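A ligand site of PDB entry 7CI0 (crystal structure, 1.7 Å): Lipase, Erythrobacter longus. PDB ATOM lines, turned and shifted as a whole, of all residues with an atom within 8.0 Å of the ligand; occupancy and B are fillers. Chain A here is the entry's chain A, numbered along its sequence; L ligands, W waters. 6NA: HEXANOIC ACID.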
ATOM      1  N   PRO A   5     -20.964  -6.189  18.004  1.00  0.00           N
ATOM      2  CA  PRO A   5     -20.087  -5.187  18.572  1.00  0.00           C
ATOM      3  C   PRO A   5     -20.843  -4.369  19.610  1.00  0.00           C
ATOM      4  O   PRO A   5     -21.986  -4.267  19.579  1.00  0.00           O
ATOM      5  CB  PRO A   5     -19.688  -4.343  17.377  1.00  0.00           C
ATOM      6  CG  PRO A   5     -20.847  -4.466  16.461  1.00  0.00           C
ATOM      7  CD  PRO A   5     -21.358  -5.874  16.659  1.00  0.00           C
ATOM      8  N   SER A 200     -10.627  -2.184   4.176  1.00  0.00           N
ATOM      9  CA  SER A 200     -10.356  -2.192   5.606  1.00  0.00           C
ATOM     10  C   SER A 200     -11.360  -3.074   6.338  1.00  0.00           C
ATOM     11  O   SER A 200     -12.489  -3.266   5.890  1.00  0.00           O
ATOM     12  CB  SER A 200     -10.405  -0.765   6.169  1.00  0.00           C
ATOM     13  OG  SER A 200     -11.735  -0.248   6.104  1.00  0.00           O
ATOM     14  N   ALA A 201     -10.925  -3.607   7.489  1.00  0.00           N
ATOM     15  CA  ALA A 201     -11.813  -4.464   8.260  1.00  0.00           C
ATOM     16  C   ALA A 201     -13.004  -3.682   8.787  1.00  0.00           C
ATOM     17  O   ALA A 201     -14.128  -4.204   8.806  1.00  0.00           O
ATOM     18  CB  ALA A 201     -11.047  -5.120   9.413  1.00  0.00           C
ATOM     19  N   SER A 202     -12.779  -2.437   9.231  1.00  0.00           N
ATOM     20  CA  SER A 202     -13.890  -1.644   9.753  1.00  0.00           C
ATOM     21  C   SER A 202     -14.939  -1.377   8.677  1.00  0.00           C
ATOM     22  O   SER A 202     -16.131  -1.374   8.958  1.00  0.00           O
ATOM     23  CB  SER A 202     -13.381  -0.337  10.378  1.00  0.00           C
ATOM     24  OG  SER A 202     -12.679   0.480   9.450  1.00  0.00           O
ATOM     25  N   LEU A 203     -14.501  -1.156   7.439  1.00  0.00           N
ATOM     26  CA  LEU A 203     -15.482  -0.883   6.387  1.00  0.00           C
ATOM     27  C   LEU A 203     -16.389  -2.090   6.167  1.00  0.00           C
ATOM     28  O   LEU A 203     -17.610  -1.943   6.043  1.00  0.00           O
ATOM     29  CB  LEU A 203     -14.771  -0.493   5.087  1.00  0.00           C
ATOM     30  CG  LEU A 203     -15.738  -0.307   3.914  1.00  0.00           C
ATOM     31  CD1 LEU A 203     -16.779   0.773   4.228  1.00  0.00           C
ATOM     32  CD2 LEU A 203     -14.969   0.033   2.647  1.00  0.00           C
ATOM     33  N   GLU A 204     -15.816  -3.291   6.144  1.00  0.00           N
ATOM     34  CA  GLU A 204     -16.635  -4.498   6.004  1.00  0.00           C
ATOM     35  C   GLU A 204     -17.536  -4.714   7.225  1.00  0.00           C
ATOM     36  O   GLU A 204     -18.701  -5.106   7.073  1.00  0.00           O
ATOM     37  CB  GLU A 204     -15.739  -5.721   5.772  1.00  0.00           C
ATOM     38  CG  GLU A 204     -16.471  -7.062   5.831  1.00  0.00           C
ATOM     39  CD  GLU A 204     -15.622  -8.252   5.386  1.00  0.00           C
ATOM     40  OE1 GLU A 204     -14.574  -8.034   4.726  1.00  0.00           O
ATOM     41  OE2 GLU A 204     -16.008  -9.405   5.677  1.00  0.00           O
ATOM     42  N   ALA A 205     -17.029  -4.451   8.434  1.00  0.00           N
ATOM     43  CA  ALA A 205     -17.794  -4.728   9.641  1.00  0.00           C
ATOM     44  C   ALA A 205     -18.970  -3.770   9.816  1.00  0.00           C
ATOM     45  O   ALA A 205     -20.026  -4.168  10.336  1.00  0.00           O
ATOM     46  CB  ALA A 205     -16.884  -4.665  10.875  1.00  0.00           C
ATOM     47  N   PHE A 206     -18.826  -2.516   9.397  1.00  0.00           N
ATOM     48  CA  PHE A 206     -19.813  -1.473   9.671  1.00  0.00           C
ATOM     49  C   PHE A 206     -20.367  -0.882   8.372  1.00  0.00           C
ATOM     50  O   PHE A 206     -20.747   0.287   8.336  1.00  0.00           O
ATOM     51  CB  PHE A 206     -19.209  -0.397  10.565  1.00  0.00           C
ATOM     52  CG  PHE A 206     -18.530  -0.946  11.804  1.00  0.00           C
ATOM     53  CD1 PHE A 206     -19.249  -1.692  12.725  1.00  0.00           C
ATOM     54  CD2 PHE A 206     -17.173  -0.750  12.015  1.00  0.00           C
ATOM     55  CE1 PHE A 206     -18.625  -2.213  13.857  1.00  0.00           C
ATOM     56  CE2 PHE A 206     -16.548  -1.267  13.138  1.00  0.00           C
ATOM     57  CZ  PHE A 206     -17.273  -2.003  14.052  1.00  0.00           C
ATOM     58  N   SER A 252     -15.793   3.662  17.593  1.00  0.00           N
ATOM     59  CA  SER A 252     -15.540   2.230  17.499  1.00  0.00           C
ATOM     60  C   SER A 252     -16.416   1.538  16.458  1.00  0.00           C
ATOM     61  O   SER A 252     -16.056   0.439  16.005  1.00  0.00           O
ATOM     62  CB  SER A 252     -15.728   1.550  18.861  1.00  0.00           C
ATOM     63  OG  SER A 252     -17.107   1.524  19.242  1.00  0.00           O
ATOM     64  N   LEU A 253     -17.546   2.136  16.076  1.00  0.00           N
ATOM     65  CA  LEU A 253     -18.457   1.551  15.107  1.00  0.00           C
ATOM     66  C   LEU A 253     -18.361   2.198  13.727  1.00  0.00           C
ATOM     67  O   LEU A 253     -19.255   1.996  12.886  1.00  0.00           O
ATOM     68  CB  LEU A 253     -19.905   1.661  15.598  1.00  0.00           C
ATOM     69  CG  LEU A 253     -20.157   1.013  16.974  1.00  0.00           C
ATOM     70  CD1 LEU A 253     -21.546   1.388  17.476  1.00  0.00           C
ATOM     71  CD2 LEU A 253     -19.996  -0.504  16.896  1.00  0.00           C
ATOM     72  N   ASP A 254     -17.337   2.983  13.473  1.00  0.00           N
ATOM     73  CA  ASP A 254     -17.199   3.757  12.229  1.00  0.00           C
ATOM     74  C   ASP A 254     -16.635   2.872  11.121  1.00  0.00           C
ATOM     75  O   ASP A 254     -15.585   2.266  11.312  1.00  0.00           O
ATOM     76  CB  ASP A 254     -16.287   4.950  12.466  1.00  0.00           C
ATOM     77  CG  ASP A 254     -16.335   5.971  11.338  1.00  0.00           C
ATOM     78  OD1 ASP A 254     -16.758   5.614  10.214  1.00  0.00           O
ATOM     79  OD2 ASP A 254     -15.933   7.128  11.577  1.00  0.00           O
ATOM     80  N   ARG A 257     -13.187   3.827  10.769  1.00  0.00           N
ATOM     81  CA  ARG A 257     -12.407   3.857  12.001  1.00  0.00           C
ATOM     82  C   ARG A 257     -10.949   3.463  11.755  1.00  0.00           C
ATOM     83  O   ARG A 257     -10.031   4.062  12.337  1.00  0.00           O
ATOM     84  CB  ARG A 257     -13.048   2.919  13.019  1.00  0.00           C
ATOM     85  CG  ARG A 257     -12.216   2.607  14.250  1.00  0.00           C
ATOM     86  CD  ARG A 257     -12.745   1.332  14.905  1.00  0.00           C
ATOM     87  NE  ARG A 257     -12.249   0.147  14.186  1.00  0.00           N
ATOM     88  CZ  ARG A 257     -12.646  -1.093  14.429  1.00  0.00           C
ATOM     89  NH1 ARG A 257     -13.587  -1.335  15.337  1.00  0.00           N
ATOM     90  NH2 ARG A 257     -12.106  -2.094  13.750  1.00  0.00           N
ATOM     91  N   ASP A 258     -10.718   2.439  10.929  1.00  0.00           N
ATOM     92  CA  ASP A 258      -9.367   1.944  10.755  1.00  0.00           C
ATOM     93  C   ASP A 258      -8.481   2.949  10.033  1.00  0.00           C
ATOM     94  O   ASP A 258      -7.252   2.881  10.170  1.00  0.00           O
ATOM     95  CB  ASP A 258      -9.360   0.605  10.014  1.00  0.00           C
ATOM     96  CG  ASP A 258      -9.932  -0.539  10.848  1.00  0.00           C
ATOM     97  OD1 ASP A 258     -10.302  -0.335  12.023  1.00  0.00           O
ATOM     98  OD2 ASP A 258     -10.005  -1.664  10.326  1.00  0.00           O
ATOM     99  N   ARG A 261      -7.179   4.958  12.915  1.00  0.00           N
ATOM    100  CA  ARG A 261      -6.150   4.131  13.548  1.00  0.00           C
ATOM    101  C   ARG A 261      -4.853   4.189  12.751  1.00  0.00           C
ATOM    102  O   ARG A 261      -3.766   4.414  13.304  1.00  0.00           O
ATOM    103  CB  ARG A 261      -6.639   2.689  13.681  1.00  0.00           C
ATOM    104  CG  ARG A 261      -7.683   2.475  14.759  1.00  0.00           C
ATOM    105  CD  ARG A 261      -8.009   1.006  14.853  1.00  0.00           C
ATOM    106  NE  ARG A 261      -9.060   0.725  15.815  1.00  0.00           N
ATOM    107  CZ  ARG A 261      -9.522  -0.497  16.065  1.00  0.00           C
ATOM    108  NH1 ARG A 261      -9.002  -1.543  15.419  1.00  0.00           N
ATOM    109  NH2 ARG A 261     -10.487  -0.670  16.955  1.00  0.00           N
ATOM    110  N   GLU A 278     -10.556   6.661  20.917  1.00  0.00           N
ATOM    111  CA  GLU A 278     -11.524   5.881  20.141  1.00  0.00           C
ATOM    112  C   GLU A 278     -12.777   5.738  20.997  1.00  0.00           C
ATOM    113  O   GLU A 278     -12.777   5.006  21.996  1.00  0.00           O
ATOM    114  CB  GLU A 278     -10.949   4.531  19.717  1.00  0.00           C
ATOM    115  CG  GLU A 278     -11.977   3.658  18.938  1.00  0.00           C
ATOM    116  CD  GLU A 278     -11.327   2.468  18.242  1.00  0.00           C
ATOM    117  OE1 GLU A 278     -10.241   2.651  17.650  1.00  0.00           O
ATOM    118  OE2 GLU A 278     -11.900   1.353  18.300  1.00  0.00           O
ATOM    119  N   GLU A 280     -16.159   4.629  22.489  1.00  0.00           N
ATOM    120  CA  GLU A 280     -16.653   3.262  22.532  1.00  0.00           C
ATOM    121  C   GLU A 280     -18.166   3.221  22.403  1.00  0.00           C
ATOM    122  O   GLU A 280     -18.875   3.875  23.173  1.00  0.00           O
ATOM    123  CB  GLU A 280     -16.224   2.585  23.830  1.00  0.00           C
ATOM    124  CG  GLU A 280     -14.733   2.314  23.881  1.00  0.00           C
ATOM    125  CD  GLU A 280     -14.326   1.293  22.833  1.00  0.00           C
ATOM    126  OE1 GLU A 280     -13.223   1.428  22.267  1.00  0.00           O
ATOM    127  OE2 GLU A 280     -15.116   0.352  22.567  1.00  0.00           O
HETATM  128  CA  6NA L   1     -12.613  -5.097  16.319  1.00  0.00           C
HETATM  129  C   6NA L   1     -11.412  -4.247  16.733  1.00  0.00           C
HETATM  130  O   6NA L   1     -11.521  -3.399  17.659  1.00  0.00           O
HETATM  131  CB  6NA L   1     -13.660  -4.261  15.567  1.00  0.00           C
HETATM  132  CG  6NA L   1     -14.393  -5.115  14.537  1.00  0.00           C
HETATM  133  CD  6NA L   1     -14.196  -4.547  13.129  1.00  0.00           C
HETATM  134  C6  6NA L   1     -13.214  -5.412  12.348  1.00  0.00           C
HETATM  135  OXT 6NA L   1     -10.296  -4.390  16.153  1.00  0.00           O
HETATM  136  O   HOH W   1     -13.948  -2.329  19.092  1.00  0.00           O
HETATM  137  O   HOH W   2     -16.432  -4.524  16.764  1.00  0.00           O
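O of the ligand lies within salt-bridge range of NH1 of Arg 257 (3.7 Å). The guanidinium group (NH2) of Arg 261 is in salt-bridge range of an oxygen (O) of the ligand, at 3.0 Å.
NH2 of Arg 261 lies within salt-bridge range of OE2 of Glu 278, at 2.8 Å. The guanidinium group (NH1) of Arg 261 lies within salt-bridge range of the side-chain carboxylate (OD1) of Asp 258, 3.8 Å away. NH1 of Arg 257 is in hydrogen-bond range of O of Ser 252. NE of Arg 257 lies within salt-bridge range of OD1 of Asp 258.
Residues that only touch the ligand: Ala 201 (3.7 Å) and Ala 205 (3.5 Å). Hydrophobic or aromatic side chains that line the ligand: Ala 201 and Ala 205. Within 4 Å of the ligand: Ala 201, Ala 205, Arg 257 and Arg 261. The nearest printed residue that does not touch the ligand is Phe 206 (4.04 Å).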
